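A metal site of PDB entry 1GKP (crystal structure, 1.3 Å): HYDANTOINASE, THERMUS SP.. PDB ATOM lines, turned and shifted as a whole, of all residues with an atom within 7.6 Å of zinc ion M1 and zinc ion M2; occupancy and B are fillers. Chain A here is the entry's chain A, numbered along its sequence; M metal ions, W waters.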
ATOM      1  N   HIS A  58      20.820  12.611 -24.554  1.00  0.00           N
ATOM      2  CA  HIS A  58      22.159  12.409 -24.983  1.00  0.00           C
ATOM      3  C   HIS A  58      22.465  13.017 -26.360  1.00  0.00           C
ATOM      4  O   HIS A  58      22.198  12.383 -27.404  1.00  0.00           O
ATOM      5  CB  HIS A  58      22.479  10.906 -25.036  1.00  0.00           C
ATOM      6  CG  HIS A  58      23.926  10.579 -25.212  1.00  0.00           C
ATOM      7  ND1 HIS A  58      24.446   9.326 -24.948  1.00  0.00           N
ATOM      8  CD2 HIS A  58      24.962  11.290 -25.700  1.00  0.00           C
ATOM      9  CE1 HIS A  58      25.735   9.315 -25.251  1.00  0.00           C
ATOM     10  NE2 HIS A  58      26.099  10.488 -25.744  1.00  0.00           N
ATOM     11  N   VAL A  59      22.964  14.257 -26.382  1.00  0.00           N
ATOM     12  CA  VAL A  59      23.226  14.913 -27.665  1.00  0.00           C
ATOM     13  C   VAL A  59      24.563  15.607 -27.595  1.00  0.00           C
ATOM     14  O   VAL A  59      25.068  15.976 -26.488  1.00  0.00           O
ATOM     15  CB  VAL A  59      22.055  15.875 -28.140  1.00  0.00           C
ATOM     16  CG1 VAL A  59      20.723  15.210 -28.227  1.00  0.00           C
ATOM     17  CG2 VAL A  59      22.048  17.138 -27.238  1.00  0.00           C
ATOM     18  N   HIS A  60      25.096  15.980 -28.736  1.00  0.00           N
ATOM     19  CA  HIS A  60      26.313  16.725 -28.866  1.00  0.00           C
ATOM     20  C   HIS A  60      26.020  17.929 -29.782  1.00  0.00           C
ATOM     21  O   HIS A  60      25.644  17.743 -30.911  1.00  0.00           O
ATOM     22  CB  HIS A  60      27.447  15.923 -29.472  1.00  0.00           C
ATOM     23  CG  HIS A  60      27.900  14.825 -28.573  1.00  0.00           C
ATOM     24  ND1 HIS A  60      28.791  15.048 -27.530  1.00  0.00           N
ATOM     25  CD2 HIS A  60      27.519  13.517 -28.473  1.00  0.00           C
ATOM     26  CE1 HIS A  60      28.970  13.878 -26.884  1.00  0.00           C
ATOM     27  NE2 HIS A  60      28.227  12.921 -27.435  1.00  0.00           N
ATOM     28  N   LEU A  63      30.896  20.544 -30.031  1.00  0.00           N
ATOM     29  CA  LEU A  63      31.889  19.473 -29.870  1.00  0.00           C
ATOM     30  C   LEU A  63      33.075  19.641 -30.803  1.00  0.00           C
ATOM     31  O   LEU A  63      32.972  19.414 -32.020  1.00  0.00           O
ATOM     32  CB  LEU A  63      31.250  18.096 -30.084  1.00  0.00           C
ATOM     33  CG  LEU A  63      32.193  16.950 -29.720  1.00  0.00           C
ATOM     34  CD1 LEU A  63      32.553  16.864 -28.253  1.00  0.00           C
ATOM     35  CD2 LEU A  63      31.626  15.656 -30.175  1.00  0.00           C
ATOM     36  N   MET A  92      25.978  16.663 -23.688  1.00  0.00           N
ATOM     37  CA  MET A  92      27.246  16.335 -23.076  1.00  0.00           C
ATOM     38  C   MET A  92      28.211  17.487 -23.146  1.00  0.00           C
ATOM     39  O   MET A  92      28.607  17.904 -24.225  1.00  0.00           O
ATOM     40  CB  MET A  92      27.861  15.083 -23.773  1.00  0.00           C
ATOM     41  CG  MET A  92      26.996  13.832 -23.719  1.00  0.00           C
ATOM     42  SD  MET A  92      27.051  13.218 -22.014  1.00  0.00           S
ATOM     43  CE  MET A  92      25.974  11.792 -22.211  1.00  0.00           C
ATOM     44  N   CYS A  94      31.718  18.539 -22.766  1.00  0.00           N
ATOM     45  CA  CYS A  94      32.912  17.691 -22.954  1.00  0.00           C
ATOM     46  C   CYS A  94      34.307  18.335 -22.987  1.00  0.00           C
ATOM     47  O   CYS A  94      35.064  18.137 -23.911  1.00  0.00           O
ATOM     48  CB  CYS A  94      32.744  16.757 -24.182  1.00  0.00           C
ATOM     49  SG  CYS A  94      31.335  15.693 -24.175  1.00  0.00           S
ATOM     50  N   KCX A 149      29.506  12.891 -16.556  1.00  0.00           N
ATOM     51  CA  KCX A 149      29.783  11.977 -17.643  1.00  0.00           C
ATOM     52  CB  KCX A 149      29.627  12.654 -19.004  1.00  0.00           C
ATOM     53  CG  KCX A 149      30.142  11.838 -20.227  1.00  0.00           C
ATOM     54  CD  KCX A 149      29.311  10.560 -20.496  1.00  0.00           C
ATOM     55  CE  KCX A 149      29.722   9.897 -21.810  1.00  0.00           C
ATOM     56  NZ  KCX A 149      29.326  10.752 -22.909  1.00  0.00           N
ATOM     57  C   KCX A 149      31.211  11.551 -17.497  1.00  0.00           C
ATOM     58  O   KCX A 149      32.121  12.361 -17.347  1.00  0.00           O
ATOM     59  CX  KCX A 149      29.380  10.333 -24.169  1.00  0.00           C
ATOM     60  OQ1 KCX A 149      29.747   9.119 -24.466  1.00  0.00           O
ATOM     61  OQ2 KCX A 149      29.083  11.186 -25.086  1.00  0.00           O
ATOM     62  N   ILE A 150      31.450  10.222 -17.496  1.00  0.00           N
ATOM     63  CA  ILE A 150      32.775   9.711 -17.581  1.00  0.00           C
ATOM     64  C   ILE A 150      32.937   8.787 -18.842  1.00  0.00           C
ATOM     65  O   ILE A 150      31.972   8.298 -19.358  1.00  0.00           O
ATOM     66  CB  ILE A 150      33.289   8.943 -16.301  1.00  0.00           C
ATOM     67  CG1 ILE A 150      32.483   7.672 -16.047  1.00  0.00           C
ATOM     68  CG2 ILE A 150      33.348   9.861 -15.106  1.00  0.00           C
ATOM     69  CD1 ILE A 150      33.050   6.767 -14.938  1.00  0.00           C
ATOM     70  N   PHE A 151      34.202   8.663 -19.216  1.00  0.00           N
ATOM     71  CA  PHE A 151      34.568   7.857 -20.392  1.00  0.00           C
ATOM     72  C   PHE A 151      35.554   6.801 -19.990  1.00  0.00           C
ATOM     73  O   PHE A 151      36.582   7.098 -19.449  1.00  0.00           O
ATOM     74  CB  PHE A 151      35.237   8.750 -21.475  1.00  0.00           C
ATOM     75  CG  PHE A 151      34.315   9.792 -22.068  1.00  0.00           C
ATOM     76  CD1 PHE A 151      34.148  11.018 -21.444  1.00  0.00           C
ATOM     77  CD2 PHE A 151      33.615   9.543 -23.229  1.00  0.00           C
ATOM     78  CE1 PHE A 151      33.349  11.976 -22.032  1.00  0.00           C
ATOM     79  CE2 PHE A 151      32.749  10.487 -23.790  1.00  0.00           C
ATOM     80  CZ  PHE A 151      32.680  11.750 -23.180  1.00  0.00           C
ATOM     81  N   SER A 153      37.342   5.087 -22.176  1.00  0.00           N
ATOM     82  CA  SER A 153      37.774   5.119 -23.589  1.00  0.00           C
ATOM     83  C   SER A 153      38.555   6.369 -23.805  1.00  0.00           C
ATOM     84  O   SER A 153      38.732   7.155 -22.870  1.00  0.00           O
ATOM     85  CB  SER A 153      36.593   5.155 -24.466  1.00  0.00           C
ATOM     86  OG  SER A 153      37.041   4.601 -25.698  1.00  0.00           O
ATOM     87  N   TYR A 154      39.089   6.560 -25.012  1.00  0.00           N
ATOM     88  CA  TYR A 154      39.760   7.782 -25.444  1.00  0.00           C
ATOM     89  C   TYR A 154      40.934   8.075 -24.549  1.00  0.00           C
ATOM     90  O   TYR A 154      40.957   9.100 -23.848  1.00  0.00           O
ATOM     91  CB  TYR A 154      38.720   8.924 -25.509  1.00  0.00           C
ATOM     92  CG  TYR A 154      37.458   8.631 -26.265  1.00  0.00           C
ATOM     93  CD1 TYR A 154      37.486   8.225 -27.625  1.00  0.00           C
ATOM     94  CD2 TYR A 154      36.224   8.737 -25.661  1.00  0.00           C
ATOM     95  CE1 TYR A 154      36.382   7.980 -28.293  1.00  0.00           C
ATOM     96  CE2 TYR A 154      35.097   8.488 -26.320  1.00  0.00           C
ATOM     97  CZ  TYR A 154      35.149   8.097 -27.657  1.00  0.00           C
ATOM     98  OH  TYR A 154      33.946   7.872 -28.226  1.00  0.00           O
ATOM     99  N   ALA A 181      28.014   7.150 -18.139  1.00  0.00           N
ATOM    100  CA  ALA A 181      29.334   6.633 -18.546  1.00  0.00           C
ATOM    101  C   ALA A 181      29.303   5.934 -19.912  1.00  0.00           C
ATOM    102  O   ALA A 181      28.426   5.148 -20.220  1.00  0.00           O
ATOM    103  CB  ALA A 181      29.760   5.556 -17.515  1.00  0.00           C
ATOM    104  N   HIS A 182      30.302   6.341 -20.708  1.00  0.00           N
ATOM    105  CA  HIS A 182      30.664   5.688 -21.971  1.00  0.00           C
ATOM    106  C   HIS A 182      31.586   4.539 -21.618  1.00  0.00           C
ATOM    107  O   HIS A 182      32.691   4.724 -21.166  1.00  0.00           O
ATOM    108  CB  HIS A 182      31.337   6.708 -22.882  1.00  0.00           C
ATOM    109  CG  HIS A 182      31.887   6.120 -24.146  1.00  0.00           C
ATOM    110  ND1 HIS A 182      31.626   6.672 -25.379  1.00  0.00           N
ATOM    111  CD2 HIS A 182      32.771   5.105 -24.354  1.00  0.00           C
ATOM    112  CE1 HIS A 182      32.323   5.993 -26.285  1.00  0.00           C
ATOM    113  NE2 HIS A 182      33.012   5.016 -25.692  1.00  0.00           N
ATOM    114  N   CYS A 183      31.093   3.319 -21.835  1.00  0.00           N
ATOM    115  CA  CYS A 183      31.783   2.115 -21.351  1.00  0.00           C
ATOM    116  C   CYS A 183      32.437   1.281 -22.463  1.00  0.00           C
ATOM    117  O   CYS A 183      31.776   0.478 -23.109  1.00  0.00           O
ATOM    118  CB  CYS A 183      30.785   1.253 -20.614  1.00  0.00           C
ATOM    119  SG  CYS A 183      30.152   2.060 -19.083  1.00  0.00           S
ATOM    120  N   GLU A 184      33.716   1.540 -22.643  1.00  0.00           N
ATOM    121  CA  GLU A 184      34.552   0.688 -23.541  1.00  0.00           C
ATOM    122  C   GLU A 184      35.801   0.391 -22.686  1.00  0.00           C
ATOM    123  O   GLU A 184      35.680   0.142 -21.455  1.00  0.00           O
ATOM    124  CB  GLU A 184      34.874   1.308 -24.916  1.00  0.00           C
ATOM    125  CG  GLU A 184      33.679   1.483 -25.791  1.00  0.00           C
ATOM    126  CD  GLU A 184      34.090   2.078 -27.116  1.00  0.00           C
ATOM    127  OE1 GLU A 184      34.542   3.254 -27.075  1.00  0.00           O
ATOM    128  OE2 GLU A 184      34.023   1.353 -28.134  1.00  0.00           O
ATOM    129  N   VAL A 237      25.507   5.013 -20.939  1.00  0.00           N
ATOM    130  CA  VAL A 237      25.073   5.700 -22.175  1.00  0.00           C
ATOM    131  C   VAL A 237      25.223   4.701 -23.382  1.00  0.00           C
ATOM    132  O   VAL A 237      26.034   3.790 -23.342  1.00  0.00           O
ATOM    133  CB  VAL A 237      25.762   7.049 -22.454  1.00  0.00           C
ATOM    134  CG1 VAL A 237      25.568   7.993 -21.283  1.00  0.00           C
ATOM    135  CG2 VAL A 237      27.177   6.882 -22.769  1.00  0.00           C
ATOM    136  N   HIS A 238      24.417   4.937 -24.403  1.00  0.00           N
ATOM    137  CA  HIS A 238      24.484   4.181 -25.692  1.00  0.00           C
ATOM    138  C   HIS A 238      24.951   2.712 -25.567  1.00  0.00           C
ATOM    139  O   HIS A 238      25.965   2.343 -26.139  1.00  0.00           O
ATOM    140  CB  HIS A 238      25.313   4.904 -26.756  1.00  0.00           C
ATOM    141  CG  HIS A 238      26.664   5.337 -26.367  1.00  0.00           C
ATOM    142  ND1 HIS A 238      27.527   4.573 -25.571  1.00  0.00           N
ATOM    143  CD2 HIS A 238      27.323   6.490 -26.655  1.00  0.00           C
ATOM    144  CE1 HIS A 238      28.679   5.229 -25.478  1.00  0.00           C
ATOM    145  NE2 HIS A 238      28.583   6.433 -26.089  1.00  0.00           N
ATOM    146  N   GLU A 261      20.719   3.369 -21.027  1.00  0.00           N
ATOM    147  CA  GLU A 261      20.259   4.074 -22.251  1.00  0.00           C
ATOM    148  C   GLU A 261      20.740   3.319 -23.470  1.00  0.00           C
ATOM    149  O   GLU A 261      21.850   2.856 -23.475  1.00  0.00           O
ATOM    150  CB  GLU A 261      20.961   5.426 -22.279  1.00  0.00           C
ATOM    151  CG  GLU A 261      20.722   6.271 -23.517  1.00  0.00           C
ATOM    152  CD  GLU A 261      21.692   7.410 -23.548  1.00  0.00           C
ATOM    153  OE1 GLU A 261      22.796   7.345 -24.141  1.00  0.00           O
ATOM    154  OE2 GLU A 261      21.428   8.525 -22.875  1.00  0.00           O
ATOM    155  N   VAL A 263      20.687   4.158 -27.846  1.00  0.00           N
ATOM    156  CA  VAL A 263      20.433   5.244 -28.792  1.00  0.00           C
ATOM    157  C   VAL A 263      19.913   4.718 -30.124  1.00  0.00           C
ATOM    158  O   VAL A 263      20.244   3.586 -30.566  1.00  0.00           O
ATOM    159  CB  VAL A 263      21.666   6.139 -28.949  1.00  0.00           C
ATOM    160  CG1 VAL A 263      21.972   6.855 -27.605  1.00  0.00           C
ATOM    161  CG2 VAL A 263      22.860   5.452 -29.484  1.00  0.00           C
ATOM    162  N   MET A 286      30.400   5.506 -35.667  1.00  0.00           N
ATOM    163  CA  MET A 286      30.160   6.157 -34.351  1.00  0.00           C
ATOM    164  C   MET A 286      30.800   5.215 -33.344  1.00  0.00           C
ATOM    165  O   MET A 286      31.224   4.093 -33.652  1.00  0.00           O
ATOM    166  CB  MET A 286      28.686   6.313 -34.129  1.00  0.00           C
ATOM    167  CG  MET A 286      27.803   5.045 -34.017  1.00  0.00           C
ATOM    168  SD  MET A 286      26.228   5.299 -33.448  1.00  0.00           S
ATOM    169  CE  MET A 286      26.601   5.737 -31.675  1.00  0.00           C
ATOM    170  N   SER A 287      30.873   5.668 -32.108  1.00  0.00           N
ATOM    171  CA  SER A 287      31.304   4.765 -31.022  1.00  0.00           C
ATOM    172  C   SER A 287      30.375   4.844 -29.841  1.00  0.00           C
ATOM    173  O   SER A 287      30.114   5.962 -29.369  1.00  0.00           O
ATOM    174  CB  SER A 287      32.668   5.151 -30.527  1.00  0.00           C
ATOM    175  OG  SER A 287      33.674   5.029 -31.529  1.00  0.00           O
ATOM    176  N   PRO A 288      29.902   3.701 -29.348  1.00  0.00           N
ATOM    177  CA  PRO A 288      30.247   2.384 -29.825  1.00  0.00           C
ATOM    178  C   PRO A 288      29.778   2.176 -31.269  1.00  0.00           C
ATOM    179  O   PRO A 288      28.745   2.698 -31.639  1.00  0.00           O
ATOM    180  CB  PRO A 288      29.538   1.455 -28.827  1.00  0.00           C
ATOM    181  CG  PRO A 288      29.070   2.294 -27.771  1.00  0.00           C
ATOM    182  CD  PRO A 288      28.993   3.673 -28.206  1.00  0.00           C
ATOM    183  N   THR A 313      19.857   9.746 -28.597  1.00  0.00           N
ATOM    184  CA  THR A 313      20.394   9.714 -29.964  1.00  0.00           C
ATOM    185  C   THR A 313      21.869   9.626 -30.059  1.00  0.00           C
ATOM    186  O   THR A 313      22.395   9.034 -30.992  1.00  0.00           O
ATOM    187  CB  THR A 313      19.958  10.972 -30.829  1.00  0.00           C
ATOM    188  OG1 THR A 313      20.385  12.117 -30.078  1.00  0.00           O
ATOM    189  CG2 THR A 313      18.441  10.956 -31.105  1.00  0.00           C
ATOM    190  N   ASP A 314      22.613  10.143 -29.084  1.00  0.00           N
ATOM    191  CA  ASP A 314      24.001  10.419 -29.240  1.00  0.00           C
ATOM    192  C   ASP A 314      24.215  11.264 -30.538  1.00  0.00           C
ATOM    193  O   ASP A 314      25.153  11.089 -31.316  1.00  0.00           O
ATOM    194  CB  ASP A 314      24.885   9.184 -29.317  1.00  0.00           C
ATOM    195  CG  ASP A 314      26.326   9.490 -29.179  1.00  0.00           C
ATOM    196  OD1 ASP A 314      26.765  10.608 -28.621  1.00  0.00           O
ATOM    197  OD2 ASP A 314      27.212   8.631 -29.434  1.00  0.00           O
ATOM    198  N   HIS A 315      23.261  12.169 -30.762  1.00  0.00           N
ATOM    199  CA  HIS A 315      23.322  13.055 -31.929  1.00  0.00           C
ATOM    200  C   HIS A 315      24.644  13.640 -32.060  1.00  0.00           C
ATOM    201  O   HIS A 315      25.132  14.398 -31.181  1.00  0.00           O
ATOM    202  CB  HIS A 315      22.237  14.148 -31.779  1.00  0.00           C
ATOM    203  CG  HIS A 315      22.231  15.165 -32.856  1.00  0.00           C
ATOM    204  ND1 HIS A 315      21.742  14.892 -34.105  1.00  0.00           N
ATOM    205  CD2 HIS A 315      22.568  16.471 -32.856  1.00  0.00           C
ATOM    206  CE1 HIS A 315      21.802  15.983 -34.843  1.00  0.00           C
ATOM    207  NE2 HIS A 315      22.364  16.933 -34.136  1.00  0.00           N
ATOM    208  N   CYS A 316      25.245  13.483 -33.255  1.00  0.00           N
ATOM    209  CA  CYS A 316      26.595  13.972 -33.324  1.00  0.00           C
ATOM    210  C   CYS A 316      26.872  14.196 -34.854  1.00  0.00           C
ATOM    211  O   CYS A 316      27.463  13.307 -35.480  1.00  0.00           O
ATOM    212  CB  CYS A 316      27.596  13.026 -32.731  1.00  0.00           C
ATOM    213  SG  CYS A 316      29.185  13.838 -32.404  1.00  0.00           S
HETATM  214 ZN    ZN M   1      27.977  10.867 -26.845  1.00  0.00          ZN
HETATM  215 ZN    ZN M   2      30.162   8.086 -26.153  1.00  0.00          ZN
HETATM  216  O   HOH W   1      28.942   9.203 -27.398  1.00  0.00           O
HETATM  217  O   HOH W   2      31.828   9.048 -27.147  1.00  0.00           O
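Of the 26 residues printed, 4 come within 4 Å of zinc ion M1.
Along chain A the residues within 4 Å of zinc ion M1 span positions 58 to 314.
The nearest printed residue that does not touch zinc ion M1 is Met 92 (4.4 Å).
Zinc ion M1 is bound by water W1 (2.0 Å), OQ2 of KCX 149 (2.1 Å), a ring nitrogen (NE2) of His 60 (2.2 Å), the side-chain carboxylate of Asp 314 (2.2 Å) and a ring nitrogen (NE2) of His 58 (2.2 Å).
Zinc ion M1 has five donor atoms within binding distance.
Zinc ion M2 is bound by OQ1 of KCX 149, water W1, water W2, ND1 of His 182 and NE2 of His 238.
Zinc ion M2 has five donor atoms within binding distance.
NZ of KCX 149 is in hydrogen-bond range of the side-chain sulfur of Met 92, 3.5 Å away.
The backbone carbonyl oxygen (O) of His 315 lies within hydrogen-bond range of the backbone NH (N) of His 60 (2.9 Å).
NE2 of His 182 is in hydrogen-bond range of OE1 of Glu 184, 2.7 Å away.
N of His 182 sits at hydrogen-bond distance from O of Ile 150 (2.9 Å).
A ring nitrogen (ND1) of His 58 sits at hydrogen-bond distance from the side-chain carboxylate (OE1) of Glu 261 (2.7 Å).
The backbone carbonyl oxygen (O) of His 58 lies within hydrogen-bond range of the side-chain hydroxyl (OG1) of Thr 313.
The backbone NH of His 238 lies within hydrogen-bond range of the side-chain carboxylate of Glu 261, 2.9 Å away.
Ser 287 touches zinc ion M2 (O to ZN, 3.9 Å).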
